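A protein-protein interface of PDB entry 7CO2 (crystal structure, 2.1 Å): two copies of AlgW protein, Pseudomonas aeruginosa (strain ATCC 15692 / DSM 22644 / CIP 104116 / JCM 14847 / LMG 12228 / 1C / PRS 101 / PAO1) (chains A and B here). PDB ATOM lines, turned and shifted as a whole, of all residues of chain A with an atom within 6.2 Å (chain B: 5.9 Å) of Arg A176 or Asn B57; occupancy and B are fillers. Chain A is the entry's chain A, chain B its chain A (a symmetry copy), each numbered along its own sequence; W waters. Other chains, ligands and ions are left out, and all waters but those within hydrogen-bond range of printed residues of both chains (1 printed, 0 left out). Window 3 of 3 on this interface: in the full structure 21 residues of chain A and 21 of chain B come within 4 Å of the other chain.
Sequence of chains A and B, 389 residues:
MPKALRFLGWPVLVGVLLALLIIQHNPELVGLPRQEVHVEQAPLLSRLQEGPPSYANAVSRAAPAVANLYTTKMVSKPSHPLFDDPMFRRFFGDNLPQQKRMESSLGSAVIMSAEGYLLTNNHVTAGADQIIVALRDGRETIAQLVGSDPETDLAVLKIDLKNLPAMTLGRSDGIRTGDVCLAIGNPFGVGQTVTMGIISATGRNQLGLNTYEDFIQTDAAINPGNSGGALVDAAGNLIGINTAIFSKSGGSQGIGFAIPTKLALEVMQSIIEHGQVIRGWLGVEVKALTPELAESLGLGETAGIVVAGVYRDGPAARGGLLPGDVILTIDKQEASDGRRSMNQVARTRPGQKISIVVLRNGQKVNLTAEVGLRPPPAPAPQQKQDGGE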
ATOM      1  N   ASP A 173     -14.023   9.522  -3.202  1.00  0.00           N
ATOM      2  CA  ASP A 173     -14.734  10.791  -3.372  1.00  0.00           C
ATOM      3  C   ASP A 173     -14.647  11.656  -2.123  1.00  0.00           C
ATOM      4  O   ASP A 173     -14.601  12.892  -2.212  1.00  0.00           O
ATOM      5  CB  ASP A 173     -16.214  10.548  -3.698  1.00  0.00           C
ATOM      6  CG  ASP A 173     -16.418   9.854  -5.030  1.00  0.00           C
ATOM      7  OD1 ASP A 173     -15.710  10.224  -5.987  1.00  0.00           O
ATOM      8  OD2 ASP A 173     -17.289   8.947  -5.112  1.00  0.00           O
ATOM      9  N   GLY A 174     -14.655  11.025  -0.958  1.00  0.00           N
ATOM     10  CA  GLY A 174     -14.698  11.730   0.293  1.00  0.00           C
ATOM     11  C   GLY A 174     -13.356  12.220   0.784  1.00  0.00           C
ATOM     12  O   GLY A 174     -13.305  12.831   1.856  1.00  0.00           O
ATOM     13  N   ILE A 175     -12.271  11.971   0.048  1.00  0.00           N
ATOM     14  CA  ILE A 175     -10.974  12.419   0.539  1.00  0.00           C
ATOM     15  C   ILE A 175     -10.812  13.899   0.233  1.00  0.00           C
ATOM     16  O   ILE A 175     -11.348  14.412  -0.761  1.00  0.00           O
ATOM     17  CB  ILE A 175      -9.815  11.601  -0.052  1.00  0.00           C
ATOM     18  CG1 ILE A 175      -9.480  12.055  -1.453  1.00  0.00           C
ATOM     19  CG2 ILE A 175     -10.138  10.118  -0.006  1.00  0.00           C
ATOM     20  CD1 ILE A 175      -8.228  11.405  -1.993  1.00  0.00           C
ATOM     21  N   ARG A 176     -10.095  14.598   1.108  1.00  0.00           N
ATOM     22  CA  ARG A 176      -9.799  16.001   0.914  1.00  0.00           C
ATOM     23  C   ARG A 176      -8.302  16.186   1.010  1.00  0.00           C
ATOM     24  O   ARG A 176      -7.631  15.507   1.794  1.00  0.00           O
ATOM     25  CB  ARG A 176     -10.476  16.905   1.969  1.00  0.00           C
ATOM     26  CG  ARG A 176     -11.950  16.659   2.226  1.00  0.00           C
ATOM     27  CD  ARG A 176     -12.457  17.572   3.314  1.00  0.00           C
ATOM     28  NE  ARG A 176     -12.408  18.952   2.866  1.00  0.00           N
ATOM     29  CZ  ARG A 176     -12.421  20.003   3.680  1.00  0.00           C
ATOM     30  NH1 ARG A 176     -12.475  19.836   4.997  1.00  0.00           N
ATOM     31  NH2 ARG A 176     -12.372  21.231   3.171  1.00  0.00           N
ATOM     32  N   THR A 177      -7.797  17.132   0.228  1.00  0.00           N
ATOM     33  CA  THR A 177      -6.439  17.594   0.395  1.00  0.00           C
ATOM     34  C   THR A 177      -6.200  17.955   1.850  1.00  0.00           C
ATOM     35  O   THR A 177      -7.056  18.555   2.508  1.00  0.00           O
ATOM     36  CB  THR A 177      -6.208  18.785  -0.522  1.00  0.00           C
ATOM     37  OG1 THR A 177      -6.418  18.326  -1.853  1.00  0.00           O
ATOM     38  CG2 THR A 177      -4.796  19.364  -0.386  1.00  0.00           C
ATOM     39  N   GLY A 178      -5.023  17.574   2.353  1.00  0.00           N
ATOM     40  CA  GLY A 178      -4.654  17.703   3.747  1.00  0.00           C
ATOM     41  C   GLY A 178      -5.010  16.509   4.614  1.00  0.00           C
ATOM     42  O   GLY A 178      -4.446  16.367   5.681  1.00  0.00           O
ATOM     43  N   ASP A 179      -5.952  15.672   4.200  1.00  0.00           N
ATOM     44  CA  ASP A 179      -6.197  14.421   4.917  1.00  0.00           C
ATOM     45  C   ASP A 179      -4.903  13.613   5.031  1.00  0.00           C
ATOM     46  O   ASP A 179      -4.080  13.636   4.125  1.00  0.00           O
ATOM     47  CB  ASP A 179      -7.245  13.600   4.184  1.00  0.00           C
ATOM     48  CG  ASP A 179      -8.664  14.023   4.510  1.00  0.00           C
ATOM     49  OD1 ASP A 179      -8.863  14.836   5.430  1.00  0.00           O
ATOM     50  OD2 ASP A 179      -9.594  13.522   3.864  1.00  0.00           O
ATOM     51  N   VAL A 180      -4.720  12.876   6.140  1.00  0.00           N
ATOM     52  CA  VAL A 180      -3.519  12.060   6.294  1.00  0.00           C
ATOM     53  C   VAL A 180      -3.704  10.735   5.553  1.00  0.00           C
ATOM     54  O   VAL A 180      -4.811  10.205   5.457  1.00  0.00           O
ATOM     55  CB  VAL A 180      -3.186  11.824   7.777  1.00  0.00           C
ATOM     56  CG1 VAL A 180      -2.109  10.757   7.911  1.00  0.00           C
ATOM     57  CG2 VAL A 180      -2.732  13.091   8.428  1.00  0.00           C
ATOM     58  N   ILE A 199      -2.714  13.834   1.642  1.00  0.00           N
ATOM     59  CA  ILE A 199      -3.196  14.016   0.272  1.00  0.00           C
ATOM     60  C   ILE A 199      -2.694  15.385  -0.163  1.00  0.00           C
ATOM     61  O   ILE A 199      -3.049  16.397   0.458  1.00  0.00           O
ATOM     62  CB  ILE A 199      -4.728  13.946   0.189  1.00  0.00           C
ATOM     63  CG1 ILE A 199      -5.263  12.665   0.813  1.00  0.00           C
ATOM     64  CG2 ILE A 199      -5.212  14.063  -1.246  1.00  0.00           C
ATOM     65  CD1 ILE A 199      -4.587  11.445   0.308  1.00  0.00           C
ATOM     66  N   THR A 202      -5.946  16.142  -5.458  1.00  0.00           N
ATOM     67  CA  THR A 202      -6.785  15.080  -5.997  1.00  0.00           C
ATOM     68  C   THR A 202      -7.095  15.410  -7.445  1.00  0.00           C
ATOM     69  O   THR A 202      -6.920  16.548  -7.891  1.00  0.00           O
ATOM     70  CB  THR A 202      -8.071  14.901  -5.170  1.00  0.00           C
ATOM     71  OG1 THR A 202      -8.936  16.002  -5.400  1.00  0.00           O
ATOM     72  CG2 THR A 202      -7.734  14.867  -3.680  1.00  0.00           C
ATOM     73  N   SER B  54      -6.547  15.326  10.401  1.00  0.00           N
ATOM     74  CA  SER B  54      -6.653  15.885   9.057  1.00  0.00           C
ATOM     75  C   SER B  54      -6.290  17.351   9.070  1.00  0.00           C
ATOM     76  O   SER B  54      -6.689  18.089   9.974  1.00  0.00           O
ATOM     77  CB  SER B  54      -8.058  15.730   8.479  1.00  0.00           C
ATOM     78  OG  SER B  54      -8.185  16.409   7.248  1.00  0.00           O
ATOM     79  N   TYR B  55      -5.565  17.781   8.043  1.00  0.00           N
ATOM     80  CA  TYR B  55      -5.245  19.193   7.881  1.00  0.00           C
ATOM     81  C   TYR B  55      -6.091  19.849   6.797  1.00  0.00           C
ATOM     82  O   TYR B  55      -5.805  20.981   6.400  1.00  0.00           O
ATOM     83  CB  TYR B  55      -3.734  19.364   7.620  1.00  0.00           C
ATOM     84  CG  TYR B  55      -2.933  18.749   8.751  1.00  0.00           C
ATOM     85  CD1 TYR B  55      -2.717  19.436   9.945  1.00  0.00           C
ATOM     86  CD2 TYR B  55      -2.466  17.436   8.658  1.00  0.00           C
ATOM     87  CE1 TYR B  55      -2.009  18.843  11.006  1.00  0.00           C
ATOM     88  CE2 TYR B  55      -1.769  16.845   9.696  1.00  0.00           C
ATOM     89  CZ  TYR B  55      -1.540  17.550  10.862  1.00  0.00           C
ATOM     90  OH  TYR B  55      -0.850  16.899  11.849  1.00  0.00           O
ATOM     91  N   ALA B  56      -7.163  19.175   6.346  1.00  0.00           N
ATOM     92  CA  ALA B  56      -7.986  19.684   5.248  1.00  0.00           C
ATOM     93  C   ALA B  56      -8.565  21.061   5.553  1.00  0.00           C
ATOM     94  O   ALA B  56      -8.635  21.908   4.669  1.00  0.00           O
ATOM     95  CB  ALA B  56      -9.124  18.708   4.938  1.00  0.00           C
ATOM     96  N   ASN B  57      -9.025  21.300   6.789  1.00  0.00           N
ATOM     97  CA  ASN B  57      -9.585  22.610   7.118  1.00  0.00           C
ATOM     98  C   ASN B  57      -8.547  23.701   6.929  1.00  0.00           C
ATOM     99  O   ASN B  57      -8.825  24.728   6.296  1.00  0.00           O
ATOM    100  CB  ASN B  57     -10.160  22.600   8.534  1.00  0.00           C
ATOM    101  CG  ASN B  57     -11.525  21.870   8.620  1.00  0.00           C
ATOM    102  OD1 ASN B  57     -12.116  21.500   7.585  1.00  0.00           O
ATOM    103  ND2 ASN B  57     -12.034  21.684   9.831  1.00  0.00           N
ATOM    104  N   ALA B  58      -7.320  23.464   7.404  1.00  0.00           N
ATOM    105  CA  ALA B  58      -6.198  24.376   7.151  1.00  0.00           C
ATOM    106  C   ALA B  58      -5.999  24.605   5.660  1.00  0.00           C
ATOM    107  O   ALA B  58      -5.862  25.743   5.201  1.00  0.00           O
ATOM    108  CB  ALA B  58      -4.915  23.820   7.771  1.00  0.00           C
ATOM    109  N   VAL B  59      -5.996  23.533   4.875  1.00  0.00           N
ATOM    110  CA  VAL B  59      -5.852  23.674   3.429  1.00  0.00           C
ATOM    111  C   VAL B  59      -6.986  24.518   2.853  1.00  0.00           C
ATOM    112  O   VAL B  59      -6.775  25.387   1.993  1.00  0.00           O
ATOM    113  CB  VAL B  59      -5.783  22.281   2.788  1.00  0.00           C
ATOM    114  CG1 VAL B  59      -6.075  22.348   1.256  1.00  0.00           C
ATOM    115  CG2 VAL B  59      -4.440  21.626   3.121  1.00  0.00           C
ATOM    116  N   SER B  60      -8.213  24.259   3.295  1.00  0.00           N
ATOM    117  CA  SER B  60      -9.349  24.981   2.724  1.00  0.00           C
ATOM    118  C   SER B  60      -9.245  26.467   3.016  1.00  0.00           C
ATOM    119  O   SER B  60      -9.617  27.303   2.189  1.00  0.00           O
ATOM    120  CB  SER B  60     -10.650  24.396   3.260  1.00  0.00           C
ATOM    121  OG  SER B  60     -10.878  23.159   2.613  1.00  0.00           O
ATOM    122  N   ARG B  61      -8.721  26.813   4.183  1.00  0.00           N
ATOM    123  CA  ARG B  61      -8.574  28.209   4.549  1.00  0.00           C
ATOM    124  C   ARG B  61      -7.521  28.883   3.684  1.00  0.00           C
ATOM    125  O   ARG B  61      -7.745  29.970   3.158  1.00  0.00           O
ATOM    126  CB  ARG B  61      -8.217  28.279   6.034  1.00  0.00           C
ATOM    127  CG  ARG B  61      -8.701  29.462   6.770  1.00  0.00           C
ATOM    128  CD  ARG B  61      -8.249  29.338   8.223  1.00  0.00           C
ATOM    129  NE  ARG B  61      -8.474  30.552   9.008  1.00  0.00           N
ATOM    130  CZ  ARG B  61      -7.841  30.815  10.146  1.00  0.00           C
ATOM    131  NH1 ARG B  61      -8.108  31.931  10.817  1.00  0.00           N
ATOM    132  NH2 ARG B  61      -6.944  29.952  10.622  1.00  0.00           N
ATOM    133  N   ALA B  62      -6.366  28.237   3.501  1.00  0.00           N
ATOM    134  CA  ALA B  62      -5.168  28.923   3.026  1.00  0.00           C
ATOM    135  C   ALA B  62      -4.944  28.786   1.535  1.00  0.00           C
ATOM    136  O   ALA B  62      -4.487  29.738   0.896  1.00  0.00           O
ATOM    137  CB  ALA B  62      -3.932  28.388   3.754  1.00  0.00           C
ATOM    138  N   ALA B 235      -3.323  25.565  11.525  1.00  0.00           N
ATOM    139  CA  ALA B 235      -4.643  26.173  11.475  1.00  0.00           C
ATOM    140  C   ALA B 235      -4.893  26.936  10.184  1.00  0.00           C
ATOM    141  O   ALA B 235      -5.993  27.481  10.007  1.00  0.00           O
ATOM    142  CB  ALA B 235      -4.839  27.133  12.660  1.00  0.00           C
HETATM  143  O   HOH W   1      -9.068  20.644   2.099  1.00  0.00           O
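The guanidinium group (NH1) of Arg A176 is in hydrogen-bond range of the side-chain amide oxygen (OD1) of Asn B57. The side-chain hydroxyl of Ser B54 sits at hydrogen-bond distance from the side-chain carboxylate of Asp A179. OG of Ser B60 is in hydrogen-bond range of NH2 of Arg A176, 2.5 Å away. The backbone carbonyl oxygen (O) of Gly A178 sits at hydrogen-bond distance from the backbone NH (N) of Tyr B55, at 3.0 Å.
The backbone carbonyl oxygen (O) of Ile A199 is in hydrogen-bond range of the backbone NH (N) of Gly A178, 3.0 Å away. The backbone NH of Arg A176 lies within hydrogen-bond range of the side-chain carboxylate of Asp A179 (3.0 Å). N of Ala B56 is in hydrogen-bond range of OG of Ser B54 (3.1 Å). The backbone carbonyl oxygen of Asp A179 is in hydrogen-bond range of the backbone NH of Ile A199 (2.8 Å). O of Ala B56 lies within hydrogen-bond range of OG of Ser B60 (3.3 Å).
Among the printed residues, merely in contact across the chains: Thr A177 with Ala B56 (3.1 Å), Arg A176 with Ala B56 (3.5 Å), Thr A177 with Val B59 (3.6 Å), Gly A178 with Ala B56 (3.8 Å), Asp A179 with Ala B56 (3.9 Å), Gly A178 with Val B59 (3.98 Å) and Gly A178 with Ser B54 (3.98 Å).
Arg A176 touches three residues of chain B. Of chain A, only Arg A176 (3.1 Å) comes within 4 Å of Asn B57. Printed residues of chain A within 4 Å of Tyr B55: Gly A178. Printed residues of chain B within 4 Å of Thr A177: Ala B56 and Val B59. The nearest residue of chain B that does not touch Arg A176 is Ser B54 (5.6 Å). The nearest printed residue of chain B that does not touch Asp A179 is Tyr B55 (4.4 Å).
Of the 10 printed residues of chain B, 6 touch a printed residue of chain A. Hydrophobic or aromatic side chains of chain B within 4 Å of the printed part of chain A: Tyr B55, Ala B56 and Val B59. Of the 10 printed residues of chain A, 4 touch a printed residue of chain B. Among the printed residues, no Asp or Glu carboxylate lies within 4 Å of a Lys or Arg side-chain nitrogen of the other chain.
No position is printed for both chains. Of the 11 pairs that touch across the chains among the printed residues, none has its exchanged pair printed and touching as well.
Water W1 lies within hydrogen-bond range of O of Ala B56 (2.9 Å), O of Thr A177 (2.9 Å) and OG of Ser B60 (3.1 Å).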
